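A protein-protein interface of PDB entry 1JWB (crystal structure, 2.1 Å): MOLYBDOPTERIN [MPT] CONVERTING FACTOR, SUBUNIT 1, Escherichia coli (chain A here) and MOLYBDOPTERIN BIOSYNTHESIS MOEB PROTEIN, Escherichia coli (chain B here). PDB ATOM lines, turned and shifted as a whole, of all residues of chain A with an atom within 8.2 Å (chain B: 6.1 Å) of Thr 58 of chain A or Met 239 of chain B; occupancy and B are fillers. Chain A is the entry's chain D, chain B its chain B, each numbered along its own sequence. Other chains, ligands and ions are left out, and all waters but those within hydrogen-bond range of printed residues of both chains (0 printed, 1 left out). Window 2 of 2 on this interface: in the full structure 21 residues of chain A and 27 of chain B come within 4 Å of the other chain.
Of the 15 printed residues of chain A, 5 touch a printed residue of chain B.
Printed residues of chain A that touch a printed residue of chain B: Ala 54, Gln 57, Thr 58, Leu 59 and Phe 75.
Hydrophobic or aromatic side chains of chain A that line the printed part of chain B: Ala 54, Leu 59 and Phe 75.
Along chain A the printed residues that touch a printed residue of chain B span positions 54 to 75.
Of the 13 printed residues of chain B, 3 touch a printed residue of chain A.
Printed residues of chain B that touch a printed residue of chain A: Met 236, Lys 237 and Met 239.
Hydrophobic or aromatic side chains of chain B within 4 Å of the printed part of chain A: Met 236 and Met 239.
Among the printed residues, no Asp or Glu carboxylate lies within 4 Å of a Lys or Arg side-chain nitrogen of the other chain.
The backbone carbonyl oxygen of Gln 57 of chain A sits at hydrogen-bond distance from the backbone NH of Lys 237 of chain B, at 2.8 Å.
O of Lys 237 of chain B sits at hydrogen-bond distance from N of Leu 59 of chain A (2.8 Å).
Thr 58 of chain A touches just these residues of chain B: Lys 237 (3.5 Å) and Met 239 (3.7 Å).
Printed residues of chain B within 4 Å of Leu 59 of chain A: Met 236 and Lys 237.
Of the printed residues of chain B, Gln 57 of chain A touches Met 236 and Lys 237.
Printed residues of chain A within 4 Å of Lys 237 of chain B: Gln 57 (2.8 Å), Thr 58 (3.5 Å) and Leu 59 (2.8 Å).
Of the printed residues of chain B, Phe 75 of chain A touches Met 236.
Of the printed residues of chain A, Met 236 of chain B touches Ala 54, Gln 57, Leu 59 and Phe 75.
Val 72 of chain A touches none of the printed residues of chain B.
The nearest printed residue of chain A that does not touch Met 236 of chain B is Ala 73 of chain A (4.6 Å).
Among the printed residues, pairs that only touch across the chains: Ala 54 of chain A with Met 236 of chain B (3.8 Å), Gln 57 of chain A with Met 236 of chain B (3.4 Å), Thr 58 of chain A with Lys 237 of chain B (3.5 Å), Thr 58 of chain A with Met 239 of chain B (3.7 Å), Leu 59 of chain A with Met 236 of chain B (3.7 Å) and Phe 75 of chain A with Met 236 of chain B (3.5 Å).
The backbone NH (N) of Ala 54 of chain A is in hydrogen-bond range of the backbone carbonyl oxygen (O) of Ala 73 of chain A (3.0 Å).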
ATOM      1  N   VAL A  28      17.196  16.423 -25.834  1.00  0.00           N
ATOM      2  CA  VAL A  28      16.911  17.320 -24.748  1.00  0.00           C
ATOM      3  C   VAL A  28      17.975  17.246 -23.647  1.00  0.00           C
ATOM      4  O   VAL A  28      18.448  18.266 -23.184  1.00  0.00           O
ATOM      5  CB  VAL A  28      15.495  17.074 -24.203  1.00  0.00           C
ATOM      6  CG1 VAL A  28      15.152  18.147 -23.183  1.00  0.00           C
ATOM      7  CG2 VAL A  28      14.502  17.116 -25.364  1.00  0.00           C
ATOM      8  N   ALA A  53      10.701  19.498 -19.510  1.00  0.00           N
ATOM      9  CA  ALA A  53      10.943  19.793 -20.902  1.00  0.00           C
ATOM     10  C   ALA A  53       9.830  19.280 -21.756  1.00  0.00           C
ATOM     11  O   ALA A  53       9.342  18.172 -21.550  1.00  0.00           O
ATOM     12  CB  ALA A  53      12.261  19.127 -21.319  1.00  0.00           C
ATOM     13  N   ALA A  54       9.391  20.113 -22.685  1.00  0.00           N
ATOM     14  CA  ALA A  54       8.454  19.689 -23.702  1.00  0.00           C
ATOM     15  C   ALA A  54       9.132  19.786 -25.089  1.00  0.00           C
ATOM     16  O   ALA A  54       9.890  20.739 -25.342  1.00  0.00           O
ATOM     17  CB  ALA A  54       7.249  20.572 -23.680  1.00  0.00           C
ATOM     18  N   VAL A  55       8.886  18.824 -25.985  1.00  0.00           N
ATOM     19  CA  VAL A  55       9.359  18.988 -27.368  1.00  0.00           C
ATOM     20  C   VAL A  55       8.121  19.081 -28.174  1.00  0.00           C
ATOM     21  O   VAL A  55       7.256  18.219 -28.088  1.00  0.00           O
ATOM     22  CB  VAL A  55      10.236  17.847 -27.961  1.00  0.00           C
ATOM     23  CG1 VAL A  55      10.989  18.368 -29.178  1.00  0.00           C
ATOM     24  CG2 VAL A  55      11.215  17.348 -27.003  1.00  0.00           C
ATOM     25  N   ASN A  56       8.028  20.166 -28.913  1.00  0.00           N
ATOM     26  CA  ASN A  56       6.909  20.453 -29.764  1.00  0.00           C
ATOM     27  C   ASN A  56       5.549  20.327 -29.118  1.00  0.00           C
ATOM     28  O   ASN A  56       4.675  19.620 -29.622  1.00  0.00           O
ATOM     29  CB  ASN A  56       7.016  19.626 -31.052  1.00  0.00           C
ATOM     30  CG  ASN A  56       8.108  20.169 -31.979  1.00  0.00           C
ATOM     31  OD1 ASN A  56       7.972  21.277 -32.537  1.00  0.00           O
ATOM     32  ND2 ASN A  56       9.211  19.433 -32.095  1.00  0.00           N
ATOM     33  N   GLN A  57       5.387  21.029 -27.990  1.00  0.00           N
ATOM     34  CA  GLN A  57       4.102  21.134 -27.282  1.00  0.00           C
ATOM     35  C   GLN A  57       3.694  19.838 -26.508  1.00  0.00           C
ATOM     36  O   GLN A  57       2.607  19.719 -25.957  1.00  0.00           O
ATOM     37  CB  GLN A  57       3.026  21.661 -28.263  1.00  0.00           C
ATOM     38  CG  GLN A  57       3.119  23.211 -28.443  1.00  0.00           C
ATOM     39  CD  GLN A  57       2.105  23.831 -29.441  1.00  0.00           C
ATOM     40  OE1 GLN A  57       0.887  23.704 -29.269  1.00  0.00           O
ATOM     41  NE2 GLN A  57       2.623  24.533 -30.454  1.00  0.00           N
ATOM     42  N   THR A  58       4.623  18.904 -26.425  1.00  0.00           N
ATOM     43  CA  THR A  58       4.405  17.639 -25.762  1.00  0.00           C
ATOM     44  C   THR A  58       5.537  17.425 -24.802  1.00  0.00           C
ATOM     45  O   THR A  58       6.691  17.626 -25.173  1.00  0.00           O
ATOM     46  CB  THR A  58       4.366  16.508 -26.815  1.00  0.00           C
ATOM     47  OG1 THR A  58       3.095  16.516 -27.475  1.00  0.00           O
ATOM     48  CG2 THR A  58       4.413  15.148 -26.134  1.00  0.00           C
ATOM     49  N   LEU A  59       5.236  17.039 -23.565  1.00  0.00           N
ATOM     50  CA  LEU A  59       6.258  16.873 -22.529  1.00  0.00           C
ATOM     51  C   LEU A  59       7.069  15.613 -22.650  1.00  0.00           C
ATOM     52  O   LEU A  59       6.512  14.540 -22.749  1.00  0.00           O
ATOM     53  CB  LEU A  59       5.619  16.791 -21.176  1.00  0.00           C
ATOM     54  CG  LEU A  59       5.125  18.076 -20.551  1.00  0.00           C
ATOM     55  CD1 LEU A  59       4.163  17.730 -19.438  1.00  0.00           C
ATOM     56  CD2 LEU A  59       6.303  18.858 -20.005  1.00  0.00           C
ATOM     57  N   VAL A  60       8.385  15.721 -22.525  1.00  0.00           N
ATOM     58  CA  VAL A  60       9.237  14.569 -22.768  1.00  0.00           C
ATOM     59  C   VAL A  60      10.290  14.387 -21.727  1.00  0.00           C
ATOM     60  O   VAL A  60      10.572  15.323 -20.961  1.00  0.00           O
ATOM     61  CB  VAL A  60       9.979  14.718 -24.099  1.00  0.00           C
ATOM     62  CG1 VAL A  60       9.151  14.224 -25.208  1.00  0.00           C
ATOM     63  CG2 VAL A  60      10.312  16.147 -24.345  1.00  0.00           C
ATOM     64  N   SER A  61      10.904  13.195 -21.717  1.00  0.00           N
ATOM     65  CA  SER A  61      11.967  12.944 -20.757  1.00  0.00           C
ATOM     66  C   SER A  61      13.254  13.546 -21.306  1.00  0.00           C
ATOM     67  O   SER A  61      13.319  13.954 -22.459  1.00  0.00           O
ATOM     68  CB  SER A  61      12.133  11.459 -20.428  1.00  0.00           C
ATOM     69  OG  SER A  61      13.045  10.806 -21.309  1.00  0.00           O
ATOM     70  N   HIS A  64      14.206  12.563 -25.171  1.00  0.00           N
ATOM     71  CA  HIS A  64      13.607  12.777 -26.464  1.00  0.00           C
ATOM     72  C   HIS A  64      14.680  13.465 -27.323  1.00  0.00           C
ATOM     73  O   HIS A  64      15.596  14.068 -26.767  1.00  0.00           O
ATOM     74  CB  HIS A  64      12.374  13.642 -26.344  1.00  0.00           C
ATOM     75  CG  HIS A  64      11.410  13.448 -27.460  1.00  0.00           C
ATOM     76  ND1 HIS A  64      10.480  12.434 -27.456  1.00  0.00           N
ATOM     77  CD2 HIS A  64      11.125  14.218 -28.539  1.00  0.00           C
ATOM     78  CE1 HIS A  64       9.641  12.622 -28.461  1.00  0.00           C
ATOM     79  NE2 HIS A  64      10.123  13.585 -29.227  1.00  0.00           N
ATOM     80  N   GLU A  71      10.637  23.006 -31.498  1.00  0.00           N
ATOM     81  CA  GLU A  71      10.470  23.974 -30.431  1.00  0.00           C
ATOM     82  C   GLU A  71      10.723  23.204 -29.145  1.00  0.00           C
ATOM     83  O   GLU A  71      10.195  22.102 -28.952  1.00  0.00           O
ATOM     84  CB  GLU A  71       9.054  24.527 -30.432  1.00  0.00           C
ATOM     85  CG  GLU A  71       8.763  25.503 -29.314  1.00  0.00           C
ATOM     86  CD  GLU A  71       7.731  26.504 -29.722  1.00  0.00           C
ATOM     87  OE1 GLU A  71       6.743  26.728 -28.971  1.00  0.00           O
ATOM     88  OE2 GLU A  71       7.919  27.075 -30.806  1.00  0.00           O
ATOM     89  N   VAL A  72      11.568  23.739 -28.280  1.00  0.00           N
ATOM     90  CA  VAL A  72      11.855  23.074 -27.026  1.00  0.00           C
ATOM     91  C   VAL A  72      11.598  24.055 -25.934  1.00  0.00           C
ATOM     92  O   VAL A  72      12.050  25.196 -26.000  1.00  0.00           O
ATOM     93  CB  VAL A  72      13.276  22.694 -26.887  1.00  0.00           C
ATOM     94  CG1 VAL A  72      13.490  22.015 -25.553  1.00  0.00           C
ATOM     95  CG2 VAL A  72      13.675  21.792 -27.990  1.00  0.00           C
ATOM     96  N   ALA A  73      10.852  23.608 -24.934  1.00  0.00           N
ATOM     97  CA  ALA A  73      10.482  24.461 -23.828  1.00  0.00           C
ATOM     98  C   ALA A  73      10.943  23.894 -22.511  1.00  0.00           C
ATOM     99  O   ALA A  73      10.707  22.734 -22.152  1.00  0.00           O
ATOM    100  CB  ALA A  73       9.022  24.693 -23.824  1.00  0.00           C
ATOM    101  N   PHE A  75      10.912  24.573 -18.442  1.00  0.00           N
ATOM    102  CA  PHE A  75      10.174  25.293 -17.443  1.00  0.00           C
ATOM    103  C   PHE A  75      10.111  24.447 -16.215  1.00  0.00           C
ATOM    104  O   PHE A  75      10.390  23.256 -16.255  1.00  0.00           O
ATOM    105  CB  PHE A  75       8.809  25.685 -17.968  1.00  0.00           C
ATOM    106  CG  PHE A  75       7.905  24.534 -18.189  1.00  0.00           C
ATOM    107  CD1 PHE A  75       6.987  24.173 -17.222  1.00  0.00           C
ATOM    108  CD2 PHE A  75       7.994  23.786 -19.352  1.00  0.00           C
ATOM    109  CE1 PHE A  75       6.146  23.092 -17.417  1.00  0.00           C
ATOM    110  CE2 PHE A  75       7.164  22.694 -19.554  1.00  0.00           C
ATOM    111  CZ  PHE A  75       6.239  22.347 -18.601  1.00  0.00           C
ATOM    112  N   GLY B 169      -4.849   4.215 -21.459  1.00  0.00           N
ATOM    113  CA  GLY B 169      -4.032   5.037 -22.338  1.00  0.00           C
ATOM    114  C   GLY B 169      -3.716   6.427 -21.867  1.00  0.00           C
ATOM    115  O   GLY B 169      -2.962   7.163 -22.505  1.00  0.00           O
ATOM    116  N   GLU B 170      -4.314   6.807 -20.749  1.00  0.00           N
ATOM    117  CA  GLU B 170      -4.081   8.118 -20.200  1.00  0.00           C
ATOM    118  C   GLU B 170      -2.939   8.066 -19.230  1.00  0.00           C
ATOM    119  O   GLU B 170      -2.798   7.130 -18.478  1.00  0.00           O
ATOM    120  CB  GLU B 170      -5.304   8.609 -19.486  1.00  0.00           C
ATOM    121  CG  GLU B 170      -5.045   9.835 -18.613  1.00  0.00           C
ATOM    122  CD  GLU B 170      -6.325  10.428 -18.090  1.00  0.00           C
ATOM    123  OE1 GLU B 170      -7.376   9.914 -18.502  1.00  0.00           O
ATOM    124  OE2 GLU B 170      -6.276  11.381 -17.276  1.00  0.00           O
ATOM    125  N   PRO B 171      -2.125   9.092 -19.228  1.00  0.00           N
ATOM    126  CA  PRO B 171      -0.986   9.109 -18.318  1.00  0.00           C
ATOM    127  C   PRO B 171      -1.502   9.342 -16.927  1.00  0.00           C
ATOM    128  O   PRO B 171      -2.592   9.868 -16.747  1.00  0.00           O
ATOM    129  CB  PRO B 171      -0.200  10.331 -18.765  1.00  0.00           C
ATOM    130  CG  PRO B 171      -1.284  11.247 -19.261  1.00  0.00           C
ATOM    131  CD  PRO B 171      -2.211  10.319 -20.053  1.00  0.00           C
ATOM    132  N   CYS B 175       3.553   9.555 -14.356  1.00  0.00           N
ATOM    133  CA  CYS B 175       4.028   9.749 -15.704  1.00  0.00           C
ATOM    134  C   CYS B 175       4.728  11.083 -15.773  1.00  0.00           C
ATOM    135  O   CYS B 175       5.674  11.272 -16.543  1.00  0.00           O
ATOM    136  CB  CYS B 175       2.894   9.752 -16.722  1.00  0.00           C
ATOM    137  SG  CYS B 175       2.301   8.116 -17.143  1.00  0.00           S
ATOM    138  N   LEU B 176       4.198  12.031 -15.000  1.00  0.00           N
ATOM    139  CA  LEU B 176       4.747  13.381 -14.901  1.00  0.00           C
ATOM    140  C   LEU B 176       5.815  13.484 -13.848  1.00  0.00           C
ATOM    141  O   LEU B 176       6.871  14.047 -14.096  1.00  0.00           O
ATOM    142  CB  LEU B 176       3.643  14.413 -14.608  1.00  0.00           C
ATOM    143  CG  LEU B 176       4.061  15.832 -14.168  1.00  0.00           C
ATOM    144  CD1 LEU B 176       5.037  16.484 -15.129  1.00  0.00           C
ATOM    145  CD2 LEU B 176       2.852  16.768 -13.957  1.00  0.00           C
ATOM    146  N   ARG B 178       7.802  11.472 -12.591  1.00  0.00           N
ATOM    147  CA  ARG B 178       9.047  10.763 -12.875  1.00  0.00           C
ATOM    148  C   ARG B 178       9.980  11.673 -13.687  1.00  0.00           C
ATOM    149  O   ARG B 178      11.167  11.408 -13.775  1.00  0.00           O
ATOM    150  CB  ARG B 178       8.853   9.320 -13.485  1.00  0.00           C
ATOM    151  CG  ARG B 178       8.185   9.081 -14.885  1.00  0.00           C
ATOM    152  CD  ARG B 178       8.400  10.131 -16.011  1.00  0.00           C
ATOM    153  NE  ARG B 178       8.658   9.555 -17.351  1.00  0.00           N
ATOM    154  CZ  ARG B 178       8.150  10.006 -18.514  1.00  0.00           C
ATOM    155  NH1 ARG B 178       7.300  11.028 -18.545  1.00  0.00           N
ATOM    156  NH2 ARG B 178       8.485   9.420 -19.662  1.00  0.00           N
ATOM    157  N   GLY B 221      -4.647  14.631 -19.984  1.00  0.00           N
ATOM    158  CA  GLY B 221      -3.667  14.470 -21.046  1.00  0.00           C
ATOM    159  C   GLY B 221      -2.793  15.688 -21.342  1.00  0.00           C
ATOM    160  O   GLY B 221      -2.098  15.740 -22.334  1.00  0.00           O
ATOM    161  N   MET B 236       0.892  21.863 -22.378  1.00  0.00           N
ATOM    162  CA  MET B 236       1.810  20.870 -22.865  1.00  0.00           C
ATOM    163  C   MET B 236       1.110  19.532 -22.740  1.00  0.00           C
ATOM    164  O   MET B 236       0.549  19.208 -21.709  1.00  0.00           O
ATOM    165  CB  MET B 236       3.007  20.839 -21.943  1.00  0.00           C
ATOM    166  CG  MET B 236       3.400  22.228 -21.404  1.00  0.00           C
ATOM    167  SD  MET B 236       4.401  22.899 -22.660  1.00  0.00           S
ATOM    168  CE  MET B 236       4.975  24.322 -21.755  1.00  0.00           C
ATOM    169  N   LYS B 237       1.160  18.734 -23.773  1.00  0.00           N
ATOM    170  CA  LYS B 237       0.524  17.438 -23.761  1.00  0.00           C
ATOM    171  C   LYS B 237       1.306  16.473 -22.906  1.00  0.00           C
ATOM    172  O   LYS B 237       2.532  16.465 -22.910  1.00  0.00           O
ATOM    173  CB  LYS B 237       0.442  16.909 -25.175  1.00  0.00           C
ATOM    174  CG  LYS B 237       0.202  15.422 -25.291  1.00  0.00           C
ATOM    175  CD  LYS B 237      -0.146  15.075 -26.735  1.00  0.00           C
ATOM    176  CE  LYS B 237      -0.795  13.745 -26.821  1.00  0.00           C
ATOM    177  NZ  LYS B 237      -1.188  13.516 -28.228  1.00  0.00           N
ATOM    178  N   LEU B 238       0.583  15.662 -22.155  1.00  0.00           N
ATOM    179  CA  LEU B 238       1.218  14.690 -21.288  1.00  0.00           C
ATOM    180  C   LEU B 238       0.930  13.308 -21.836  1.00  0.00           C
ATOM    181  O   LEU B 238      -0.233  12.918 -22.018  1.00  0.00           O
ATOM    182  CB  LEU B 238       0.701  14.852 -19.854  1.00  0.00           C
ATOM    183  CG  LEU B 238       1.125  13.899 -18.754  1.00  0.00           C
ATOM    184  CD1 LEU B 238       2.600  13.887 -18.436  1.00  0.00           C
ATOM    185  CD2 LEU B 238       0.382  14.244 -17.514  1.00  0.00           C
ATOM    186  N   MET B 239       1.994  12.591 -22.154  1.00  0.00           N
ATOM    187  CA  MET B 239       1.884  11.222 -22.632  1.00  0.00           C
ATOM    188  C   MET B 239       2.191  10.203 -21.559  1.00  0.00           C
ATOM    189  O   MET B 239       2.998  10.434 -20.671  1.00  0.00           O
ATOM    190  CB  MET B 239       2.901  11.004 -23.728  1.00  0.00           C
ATOM    191  CG  MET B 239       2.814  12.046 -24.812  1.00  0.00           C
ATOM    192  SD  MET B 239       1.455  11.738 -25.880  1.00  0.00           S
ATOM    193  CE  MET B 239       2.024  10.163 -26.613  1.00  0.00           C
ATOM    194  N   ARG B 240       1.586   9.034 -21.697  1.00  0.00           N
ATOM    195  CA  ARG B 240       1.814   7.938 -20.775  1.00  0.00           C
ATOM    196  C   ARG B 240       3.227   7.420 -20.940  1.00  0.00           C
ATOM    197  O   ARG B 240       3.659   7.211 -22.067  1.00  0.00           O
ATOM    198  CB  ARG B 240       0.848   6.809 -21.097  1.00  0.00           C
ATOM    199  CG  ARG B 240       0.817   5.675 -20.102  1.00  0.00           C
ATOM    200  CD  ARG B 240      -0.608   5.132 -19.948  1.00  0.00           C
ATOM    201  NE  ARG B 240      -0.785   4.078 -18.946  1.00  0.00           N
ATOM    202  CZ  ARG B 240      -1.961   3.752 -18.389  1.00  0.00           C
ATOM    203  NH1 ARG B 240      -3.082   4.408 -18.700  1.00  0.00           N
ATOM    204  NH2 ARG B 240      -2.004   2.772 -17.494  1.00  0.00           N
ATOM    205  N   ASN B 241       3.946   7.227 -19.837  1.00  0.00           N
ATOM    206  CA  ASN B 241       5.273   6.637 -19.898  1.00  0.00           C
ATOM    207  C   ASN B 241       5.196   5.113 -19.755  1.00  0.00           C
ATOM    208  O   ASN B 241       4.855   4.578 -18.702  1.00  0.00           O
ATOM    209  CB  ASN B 241       6.197   7.262 -18.858  1.00  0.00           C
ATOM    210  CG  ASN B 241       7.502   6.509 -18.685  1.00  0.00           C
ATOM    211  OD1 ASN B 241       7.979   6.364 -17.560  1.00  0.00           O
ATOM    212  ND2 ASN B 241       8.086   6.037 -19.781  1.00  0.00           N
